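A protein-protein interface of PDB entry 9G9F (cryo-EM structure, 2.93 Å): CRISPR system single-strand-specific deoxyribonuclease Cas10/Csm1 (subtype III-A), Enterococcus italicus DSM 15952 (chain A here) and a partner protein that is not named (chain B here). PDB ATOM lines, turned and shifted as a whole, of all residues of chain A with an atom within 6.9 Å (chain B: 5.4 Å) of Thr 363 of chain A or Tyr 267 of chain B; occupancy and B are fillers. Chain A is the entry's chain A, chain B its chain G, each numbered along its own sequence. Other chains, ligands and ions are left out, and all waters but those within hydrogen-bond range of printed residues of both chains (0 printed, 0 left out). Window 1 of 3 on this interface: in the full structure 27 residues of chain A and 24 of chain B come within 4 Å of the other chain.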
ATOM      1  N   SER A 277      -4.576   5.239  28.568  1.00  0.00           N
ATOM      2  CA  SER A 277      -5.476   6.352  28.312  1.00  0.00           C
ATOM      3  C   SER A 277      -6.234   6.104  27.019  1.00  0.00           C
ATOM      4  O   SER A 277      -5.638   5.711  26.011  1.00  0.00           O
ATOM      5  CB  SER A 277      -4.699   7.666  28.228  1.00  0.00           C
ATOM      6  OG  SER A 277      -3.753   7.759  29.278  1.00  0.00           O
ATOM      7  N   GLY A 278      -7.545   6.323  27.050  1.00  0.00           N
ATOM      8  CA  GLY A 278      -8.359   6.188  25.861  1.00  0.00           C
ATOM      9  C   GLY A 278      -8.753   4.776  25.503  1.00  0.00           C
ATOM     10  O   GLY A 278      -8.982   4.498  24.321  1.00  0.00           O
ATOM     11  N   PHE A 357       3.447   4.270  20.801  1.00  0.00           N
ATOM     12  CA  PHE A 357       2.013   4.515  20.868  1.00  0.00           C
ATOM     13  C   PHE A 357       1.615   5.679  19.977  1.00  0.00           C
ATOM     14  O   PHE A 357       0.544   5.655  19.364  1.00  0.00           O
ATOM     15  CB  PHE A 357       1.589   4.765  22.313  1.00  0.00           C
ATOM     16  CG  PHE A 357       1.182   3.522  23.042  1.00  0.00           C
ATOM     17  CD1 PHE A 357      -0.093   3.009  22.906  1.00  0.00           C
ATOM     18  CD2 PHE A 357       2.081   2.860  23.858  1.00  0.00           C
ATOM     19  CE1 PHE A 357      -0.463   1.866  23.572  1.00  0.00           C
ATOM     20  CE2 PHE A 357       1.713   1.716  24.524  1.00  0.00           C
ATOM     21  CZ  PHE A 357       0.441   1.220  24.382  1.00  0.00           C
ATOM     22  N   ILE A 358       2.459   6.708  19.892  1.00  0.00           N
ATOM     23  CA  ILE A 358       2.183   7.810  18.977  1.00  0.00           C
ATOM     24  C   ILE A 358       2.198   7.320  17.536  1.00  0.00           C
ATOM     25  O   ILE A 358       1.312   7.649  16.738  1.00  0.00           O
ATOM     26  CB  ILE A 358       3.189   8.952  19.194  1.00  0.00           C
ATOM     27  CG1 ILE A 358       2.741   9.826  20.358  1.00  0.00           C
ATOM     28  CG2 ILE A 358       3.350   9.777  17.932  1.00  0.00           C
ATOM     29  CD1 ILE A 358       3.509  11.102  20.468  1.00  0.00           C
ATOM     30  N   PHE A 361      -0.925   4.712  17.165  1.00  0.00           N
ATOM     31  CA  PHE A 361      -2.238   5.291  17.480  1.00  0.00           C
ATOM     32  C   PHE A 361      -2.017   6.745  17.890  1.00  0.00           C
ATOM     33  O   PHE A 361      -1.762   7.031  19.062  1.00  0.00           O
ATOM     34  CB  PHE A 361      -2.956   4.524  18.583  1.00  0.00           C
ATOM     35  CG  PHE A 361      -2.930   3.033  18.421  1.00  0.00           C
ATOM     36  CD1 PHE A 361      -3.880   2.390  17.654  1.00  0.00           C
ATOM     37  CD2 PHE A 361      -1.970   2.274  19.062  1.00  0.00           C
ATOM     38  CE1 PHE A 361      -3.863   1.022  17.518  1.00  0.00           C
ATOM     39  CE2 PHE A 361      -1.950   0.906  18.926  1.00  0.00           C
ATOM     40  CZ  PHE A 361      -2.896   0.280  18.154  1.00  0.00           C
ATOM     41  N   LYS A 362      -2.147   7.662  16.939  1.00  0.00           N
ATOM     42  CA  LYS A 362      -1.950   9.080  17.239  1.00  0.00           C
ATOM     43  C   LYS A 362      -3.079   9.552  18.146  1.00  0.00           C
ATOM     44  O   LYS A 362      -4.209   9.759  17.698  1.00  0.00           O
ATOM     45  CB  LYS A 362      -1.888   9.900  15.956  1.00  0.00           C
ATOM     46  CG  LYS A 362      -0.600   9.728  15.177  1.00  0.00           C
ATOM     47  CD  LYS A 362      -0.439  10.809  14.129  1.00  0.00           C
ATOM     48  CE  LYS A 362       0.942  10.763  13.505  1.00  0.00           C
ATOM     49  NZ  LYS A 362       1.159  11.898  12.569  1.00  0.00           N
ATOM     50  N   THR A 363      -2.771   9.709  19.433  1.00  0.00           N
ATOM     51  CA  THR A 363      -3.662  10.142  20.509  1.00  0.00           C
ATOM     52  C   THR A 363      -4.833   9.199  20.741  1.00  0.00           C
ATOM     53  O   THR A 363      -5.661   9.477  21.615  1.00  0.00           O
ATOM     54  CB  THR A 363      -4.221  11.558  20.297  1.00  0.00           C
ATOM     55  OG1 THR A 363      -5.368  11.502  19.441  1.00  0.00           O
ATOM     56  CG2 THR A 363      -3.170  12.477  19.691  1.00  0.00           C
ATOM     57  N   ASP A 364      -4.935   8.093  20.003  1.00  0.00           N
ATOM     58  CA  ASP A 364      -6.008   7.138  20.253  1.00  0.00           C
ATOM     59  C   ASP A 364      -5.728   6.286  21.482  1.00  0.00           C
ATOM     60  O   ASP A 364      -6.668   5.874  22.171  1.00  0.00           O
ATOM     61  CB  ASP A 364      -6.220   6.246  19.030  1.00  0.00           C
ATOM     62  CG  ASP A 364      -6.910   6.972  17.891  1.00  0.00           C
ATOM     63  OD1 ASP A 364      -7.589   7.986  18.154  1.00  0.00           O
ATOM     64  OD2 ASP A 364      -6.774   6.527  16.732  1.00  0.00           O
ATOM     65  N   LEU A 365      -4.458   6.006  21.760  1.00  0.00           N
ATOM     66  CA  LEU A 365      -4.054   5.257  22.941  1.00  0.00           C
ATOM     67  C   LEU A 365      -2.745   5.827  23.460  1.00  0.00           C
ATOM     68  O   LEU A 365      -1.926   6.345  22.697  1.00  0.00           O
ATOM     69  CB  LEU A 365      -3.894   3.766  22.640  1.00  0.00           C
ATOM     70  CG  LEU A 365      -5.175   2.950  22.510  1.00  0.00           C
ATOM     71  CD1 LEU A 365      -4.849   1.569  21.987  1.00  0.00           C
ATOM     72  CD2 LEU A 365      -5.883   2.866  23.845  1.00  0.00           C
ATOM     73  N   SER A 366      -2.552   5.720  24.770  1.00  0.00           N
ATOM     74  CA  SER A 366      -1.317   6.170  25.399  1.00  0.00           C
ATOM     75  C   SER A 366      -1.127   5.405  26.700  1.00  0.00           C
ATOM     76  O   SER A 366      -2.055   4.779  27.216  1.00  0.00           O
ATOM     77  CB  SER A 366      -1.334   7.680  25.652  1.00  0.00           C
ATOM     78  OG  SER A 366      -1.380   8.407  24.437  1.00  0.00           O
ATOM     79  N   LYS A 404       1.314  14.751  29.105  1.00  0.00           N
ATOM     80  CA  LYS A 404       1.072  13.669  28.153  1.00  0.00           C
ATOM     81  C   LYS A 404       1.806  13.780  26.818  1.00  0.00           C
ATOM     82  O   LYS A 404       1.784  12.825  26.035  1.00  0.00           O
ATOM     83  CB  LYS A 404      -0.430  13.547  27.885  1.00  0.00           C
ATOM     84  CG  LYS A 404      -0.890  12.161  27.497  1.00  0.00           C
ATOM     85  CD  LYS A 404      -2.399  12.106  27.421  1.00  0.00           C
ATOM     86  CE  LYS A 404      -2.883  10.733  27.010  1.00  0.00           C
ATOM     87  NZ  LYS A 404      -4.367  10.688  26.948  1.00  0.00           N
ATOM     88  N   TYR A 405       2.478  14.896  26.543  1.00  0.00           N
ATOM     89  CA  TYR A 405       3.147  15.062  25.256  1.00  0.00           C
ATOM     90  C   TYR A 405       4.299  16.041  25.408  1.00  0.00           C
ATOM     91  O   TYR A 405       4.415  16.747  26.411  1.00  0.00           O
ATOM     92  CB  TYR A 405       2.179  15.542  24.165  1.00  0.00           C
ATOM     93  CG  TYR A 405       1.273  14.457  23.636  1.00  0.00           C
ATOM     94  CD1 TYR A 405       1.792  13.330  23.022  1.00  0.00           C
ATOM     95  CD2 TYR A 405      -0.103  14.555  23.762  1.00  0.00           C
ATOM     96  CE1 TYR A 405       0.966  12.334  22.551  1.00  0.00           C
ATOM     97  CE2 TYR A 405      -0.934  13.565  23.290  1.00  0.00           C
ATOM     98  CZ  TYR A 405      -0.394  12.458  22.685  1.00  0.00           C
ATOM     99  OH  TYR A 405      -1.216  11.468  22.212  1.00  0.00           O
ATOM    100  N   ILE A 410       4.469  17.047  19.353  1.00  0.00           N
ATOM    101  CA  ILE A 410       3.453  17.958  18.832  1.00  0.00           C
ATOM    102  C   ILE A 410       3.843  18.465  17.450  1.00  0.00           C
ATOM    103  O   ILE A 410       3.011  18.522  16.533  1.00  0.00           O
ATOM    104  CB  ILE A 410       3.220  19.121  19.812  1.00  0.00           C
ATOM    105  CG1 ILE A 410       2.650  18.609  21.132  1.00  0.00           C
ATOM    106  CG2 ILE A 410       2.285  20.139  19.204  1.00  0.00           C
ATOM    107  CD1 ILE A 410       2.420  19.700  22.149  1.00  0.00           C
ATOM    108  N   LEU A 412       5.768  16.991  15.306  1.00  0.00           N
ATOM    109  CA  LEU A 412       5.584  15.868  14.392  1.00  0.00           C
ATOM    110  C   LEU A 412       4.115  15.696  14.031  1.00  0.00           C
ATOM    111  O   LEU A 412       3.780  15.388  12.880  1.00  0.00           O
ATOM    112  CB  LEU A 412       6.146  14.591  15.018  1.00  0.00           C
ATOM    113  CG  LEU A 412       5.814  13.249  14.357  1.00  0.00           C
ATOM    114  CD1 LEU A 412       7.076  12.420  14.181  1.00  0.00           C
ATOM    115  CD2 LEU A 412       4.780  12.480  15.168  1.00  0.00           C
ATOM    116  N   PHE A 413       3.224  15.885  15.007  1.00  0.00           N
ATOM    117  CA  PHE A 413       1.792  15.796  14.740  1.00  0.00           C
ATOM    118  C   PHE A 413       1.352  16.836  13.721  1.00  0.00           C
ATOM    119  O   PHE A 413       0.571  16.534  12.813  1.00  0.00           O
ATOM    120  CB  PHE A 413       1.005  15.975  16.036  1.00  0.00           C
ATOM    121  CG  PHE A 413       0.941  14.746  16.888  1.00  0.00           C
ATOM    122  CD1 PHE A 413       0.923  13.491  16.315  1.00  0.00           C
ATOM    123  CD2 PHE A 413       0.883  14.851  18.264  1.00  0.00           C
ATOM    124  CE1 PHE A 413       0.853  12.363  17.101  1.00  0.00           C
ATOM    125  CE2 PHE A 413       0.814  13.729  19.051  1.00  0.00           C
ATOM    126  CZ  PHE A 413       0.798  12.484  18.470  1.00  0.00           C
ATOM    127  N   ASN A 414       1.841  18.066  13.853  1.00  0.00           N
ATOM    128  CA  ASN A 414       1.382  19.164  13.012  1.00  0.00           C
ATOM    129  C   ASN A 414       2.190  19.332  11.731  1.00  0.00           C
ATOM    130  O   ASN A 414       1.966  20.303  11.002  1.00  0.00           O
ATOM    131  CB  ASN A 414       1.404  20.476  13.799  1.00  0.00           C
ATOM    132  CG  ASN A 414       0.306  20.548  14.830  1.00  0.00           C
ATOM    133  OD1 ASN A 414      -0.716  19.878  14.708  1.00  0.00           O
ATOM    134  ND2 ASN A 414       0.509  21.366  15.853  1.00  0.00           N
ATOM    135  N   THR A 416       2.222  17.206   9.039  1.00  0.00           N
ATOM    136  CA  THR A 416       1.750  16.290   8.012  1.00  0.00           C
ATOM    137  C   THR A 416       2.015  16.864   6.624  1.00  0.00           C
ATOM    138  O   THR A 416       2.053  18.082   6.426  1.00  0.00           O
ATOM    139  CB  THR A 416       0.257  16.013   8.182  1.00  0.00           C
ATOM    140  OG1 THR A 416      -0.065  15.966   9.577  1.00  0.00           O
ATOM    141  CG2 THR A 416      -0.116  14.686   7.543  1.00  0.00           C
ATOM    142  N   ASP A 431      -3.292   8.501   6.884  1.00  0.00           N
ATOM    143  CA  ASP A 431      -1.855   8.393   6.639  1.00  0.00           C
ATOM    144  C   ASP A 431      -1.416   6.938   6.510  1.00  0.00           C
ATOM    145  O   ASP A 431      -0.520   6.623   5.719  1.00  0.00           O
ATOM    146  CB  ASP A 431      -1.075   9.105   7.745  1.00  0.00           C
ATOM    147  CG  ASP A 431      -1.643   8.844   9.125  1.00  0.00           C
ATOM    148  OD1 ASP A 431      -1.614   7.681   9.576  1.00  0.00           O
ATOM    149  OD2 ASP A 431      -2.116   9.808   9.763  1.00  0.00           O
ATOM    150  N   MET B 227      -3.374  26.451  18.834  1.00  0.00           N
ATOM    151  CA  MET B 227      -2.047  25.857  18.766  1.00  0.00           C
ATOM    152  C   MET B 227      -1.085  26.906  18.236  1.00  0.00           C
ATOM    153  O   MET B 227      -1.445  27.696  17.363  1.00  0.00           O
ATOM    154  CB  MET B 227      -2.021  24.606  17.883  1.00  0.00           C
ATOM    155  CG  MET B 227      -0.625  24.072  17.604  1.00  0.00           C
ATOM    156  SD  MET B 227       0.119  23.216  18.996  1.00  0.00           S
ATOM    157  CE  MET B 227      -1.096  21.944  19.287  1.00  0.00           C
ATOM    158  N   LEU B 244      -4.618  17.435  23.867  1.00  0.00           N
ATOM    159  CA  LEU B 244      -4.505  17.518  22.415  1.00  0.00           C
ATOM    160  C   LEU B 244      -5.717  16.848  21.787  1.00  0.00           C
ATOM    161  O   LEU B 244      -5.892  15.632  21.902  1.00  0.00           O
ATOM    162  CB  LEU B 244      -3.216  16.861  21.931  1.00  0.00           C
ATOM    163  CG  LEU B 244      -2.037  17.775  21.607  1.00  0.00           C
ATOM    164  CD1 LEU B 244      -1.043  17.055  20.723  1.00  0.00           C
ATOM    165  CD2 LEU B 244      -2.509  19.041  20.944  1.00  0.00           C
ATOM    166  N   LYS B 245      -6.553  17.634  21.119  1.00  0.00           N
ATOM    167  CA  LYS B 245      -7.706  17.127  20.396  1.00  0.00           C
ATOM    168  C   LYS B 245      -7.383  17.064  18.911  1.00  0.00           C
ATOM    169  O   LYS B 245      -6.722  17.959  18.369  1.00  0.00           O
ATOM    170  CB  LYS B 245      -8.930  18.012  20.634  1.00  0.00           C
ATOM    171  CG  LYS B 245     -10.204  17.245  20.936  1.00  0.00           C
ATOM    172  CD  LYS B 245     -11.291  18.172  21.451  1.00  0.00           C
ATOM    173  CE  LYS B 245     -11.673  19.209  20.411  1.00  0.00           C
ATOM    174  NZ  LYS B 245     -12.295  18.586  19.210  1.00  0.00           N
ATOM    175  N   LYS B 246      -7.854  16.000  18.265  1.00  0.00           N
ATOM    176  CA  LYS B 246      -7.576  15.728  16.855  1.00  0.00           C
ATOM    177  C   LYS B 246      -8.643  16.399  16.001  1.00  0.00           C
ATOM    178  O   LYS B 246      -9.780  15.927  15.921  1.00  0.00           O
ATOM    179  CB  LYS B 246      -7.537  14.226  16.606  1.00  0.00           C
ATOM    180  CG  LYS B 246      -7.411  13.838  15.148  1.00  0.00           C
ATOM    181  CD  LYS B 246      -7.483  12.330  14.983  1.00  0.00           C
ATOM    182  CE  LYS B 246      -7.270  11.919  13.538  1.00  0.00           C
ATOM    183  NZ  LYS B 246      -5.914  12.281  13.053  1.00  0.00           N
ATOM    184  N   ARG B 247      -8.274  17.501  15.352  1.00  0.00           N
ATOM    185  CA  ARG B 247      -9.163  18.209  14.440  1.00  0.00           C
ATOM    186  C   ARG B 247      -8.873  17.732  13.021  1.00  0.00           C
ATOM    187  O   ARG B 247      -7.754  17.888  12.518  1.00  0.00           O
ATOM    188  CB  ARG B 247      -8.978  19.717  14.565  1.00  0.00           C
ATOM    189  CG  ARG B 247      -8.806  20.200  15.988  1.00  0.00           C
ATOM    190  CD  ARG B 247     -10.049  19.919  16.815  1.00  0.00           C
ATOM    191  NE  ARG B 247     -11.202  20.698  16.378  1.00  0.00           N
ATOM    192  CZ  ARG B 247     -12.362  20.176  16.005  1.00  0.00           C
ATOM    193  NH1 ARG B 247     -12.566  18.869  16.010  1.00  0.00           N
ATOM    194  NH2 ARG B 247     -13.343  20.985  15.619  1.00  0.00           N
ATOM    195  N   ASP B 265      -4.344  16.309   8.652  1.00  0.00           N
ATOM    196  CA  ASP B 265      -4.704  16.137  10.053  1.00  0.00           C
ATOM    197  C   ASP B 265      -4.086  17.234  10.907  1.00  0.00           C
ATOM    198  O   ASP B 265      -2.929  17.615  10.718  1.00  0.00           O
ATOM    199  CB  ASP B 265      -4.248  14.766  10.553  1.00  0.00           C
ATOM    200  CG  ASP B 265      -5.058  13.632   9.964  1.00  0.00           C
ATOM    201  OD1 ASP B 265      -5.901  13.892   9.081  1.00  0.00           O
ATOM    202  OD2 ASP B 265      -4.847  12.474  10.380  1.00  0.00           O
ATOM    203  N   PHE B 266      -4.870  17.749  11.850  1.00  0.00           N
ATOM    204  CA  PHE B 266      -4.413  18.800  12.742  1.00  0.00           C
ATOM    205  C   PHE B 266      -4.647  18.366  14.178  1.00  0.00           C
ATOM    206  O   PHE B 266      -5.558  17.587  14.463  1.00  0.00           O
ATOM    207  CB  PHE B 266      -5.135  20.118  12.456  1.00  0.00           C
ATOM    208  CG  PHE B 266      -4.507  21.312  13.106  1.00  0.00           C
ATOM    209  CD1 PHE B 266      -3.320  21.830  12.633  1.00  0.00           C
ATOM    210  CD2 PHE B 266      -5.120  21.934  14.177  1.00  0.00           C
ATOM    211  CE1 PHE B 266      -2.748  22.933  13.227  1.00  0.00           C
ATOM    212  CE2 PHE B 266      -4.553  23.039  14.771  1.00  0.00           C
ATOM    213  CZ  PHE B 266      -3.367  23.536  14.296  1.00  0.00           C
ATOM    214  N   TYR B 267      -3.809  18.863  15.082  1.00  0.00           N
ATOM    215  CA  TYR B 267      -3.941  18.581  16.506  1.00  0.00           C
ATOM    216  C   TYR B 267      -3.814  19.893  17.258  1.00  0.00           C
ATOM    217  O   TYR B 267      -2.846  20.630  17.054  1.00  0.00           O
ATOM    218  CB  TYR B 267      -2.883  17.581  16.972  1.00  0.00           C
ATOM    219  CG  TYR B 267      -3.065  16.209  16.380  1.00  0.00           C
ATOM    220  CD1 TYR B 267      -3.880  15.276  16.992  1.00  0.00           C
ATOM    221  CD2 TYR B 267      -2.429  15.851  15.205  1.00  0.00           C
ATOM    222  CE1 TYR B 267      -4.054  14.024  16.454  1.00  0.00           C
ATOM    223  CE2 TYR B 267      -2.596  14.601  14.659  1.00  0.00           C
ATOM    224  CZ  TYR B 267      -3.411  13.692  15.287  1.00  0.00           C
ATOM    225  OH  TYR B 267      -3.582  12.440  14.746  1.00  0.00           O
ATOM    226  N   ALA B 268      -4.785  20.188  18.118  1.00  0.00           N
ATOM    227  CA  ALA B 268      -4.806  21.477  18.791  1.00  0.00           C
ATOM    228  C   ALA B 268      -5.191  21.309  20.250  1.00  0.00           C
ATOM    229  O   ALA B 268      -5.914  20.381  20.614  1.00  0.00           O
ATOM    230  CB  ALA B 268      -5.773  22.450  18.110  1.00  0.00           C
ATOM    231  N   PHE B 269      -4.699  22.222  21.083  1.00  0.00           N
ATOM    232  CA  PHE B 269      -5.040  22.209  22.497  1.00  0.00           C
ATOM    233  C   PHE B 269      -6.534  22.430  22.675  1.00  0.00           C
ATOM    234  O   PHE B 269      -7.118  23.322  22.056  1.00  0.00           O
ATOM    235  CB  PHE B 269      -4.261  23.292  23.239  1.00  0.00           C
ATOM    236  CG  PHE B 269      -2.774  23.153  23.132  1.00  0.00           C
ATOM    237  CD1 PHE B 269      -2.174  21.913  23.197  1.00  0.00           C
ATOM    238  CD2 PHE B 269      -1.976  24.268  22.970  1.00  0.00           C
ATOM    239  CE1 PHE B 269      -0.809  21.789  23.099  1.00  0.00           C
ATOM    240  CE2 PHE B 269      -0.613  24.148  22.874  1.00  0.00           C
ATOM    241  CZ  PHE B 269      -0.030  22.909  22.937  1.00  0.00           C
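Thr 363 of chain A touches just one residue of chain B: Tyr 267. Of chain A, only Lys 362 (3.3 Å), Thr 363 (3.7 Å), Phe 413 (3.5 Å) and Asn 414 (3.3 Å) come within 4 Å of Tyr 267 of chain B. Printed residues of chain B within 4 Å of Thr 416 of chain A: Asp 265. Printed residues of chain A within 4 Å of Leu 244 of chain B: Phe 413 (3.8 Å). The nearest residue of chain B that does not touch Thr 363 of chain A is Lys 246 of chain B (4.5 Å). The nearest residue of chain A that does not touch Tyr 267 of chain B is Ile 410 of chain A (5.6 Å). The nearest printed residue of chain A that does not touch Asp 265 of chain B is Phe 413 of chain A (4.2 Å).
The side-chain amino group (NZ) of Lys 246 of chain B lies within salt-bridge range of the side-chain carboxylate (OD2) of Asp 265 of chain B (2.9 Å). N of Arg 247 of chain B sits at hydrogen-bond distance from O of Phe 266 of chain B (2.9 Å). The backbone carbonyl oxygen of Phe 413 of chain A lies within hydrogen-bond range of the side-chain hydroxyl of Thr 416 of chain A (3.3 Å). The side-chain amino group (NZ) of Lys 246 of chain B sits at hydrogen-bond distance from the side-chain hydroxyl (OH) of Tyr 267 of chain B (2.9 Å).
The side-chain amide nitrogen (ND2) of Asn 414 of chain A lies close to the side-chain sulfur (SD) of Met 227 of chain B (3.7 Å). The side-chain amide oxygen of Asn 414 of chain A sits close to the backbone carbonyl oxygen of Tyr 267 of chain B. The side-chain hydroxyl (OG1) of Thr 416 of chain A sits at hydrogen-bond distance from the backbone carbonyl oxygen (O) of Asp 265 of chain B, 3.5 Å away.
Printed residues of chain B that touch a printed residue of chain A: Met 227, Leu 244, Asp 265, Phe 266, Tyr 267 and Phe 269. Printed residues of chain A that touch a printed residue of chain B: Lys 362, Thr 363, Ile 410, Phe 413, Asn 414, Thr 416 and Asp 431. Hydrophobic or aromatic side chains of chain A within 4 Å of the printed part of chain B: Ile 410 and Phe 413. Along chain A the printed residues that touch a printed residue of chain B span positions 362 to 431. Among the printed residues, no Asp or Glu carboxylate lies within 4 Å of a Lys or Arg side-chain nitrogen of the other chain.
CB of Lys 362 of chain A touches OH of Tyr 267 of chain B, 3.3 Å away. Thr 363 of chain A touches Tyr 267 of chain B. Met 227 of chain B touches Ile 410 of chain A. Ile 410 of chain A touches Phe 269 of chain B. Leu 244 of chain B touches Phe 413 of chain A (CD1 to CD2, 3.8 Å). Tyr 267 of chain B touches Phe 413 of chain A. CD1 of Phe 266 of chain B touches OD1 of Asn 414 of chain A, at 3.9 Å. Asp 431 of chain A touches Asp 265 of chain B.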
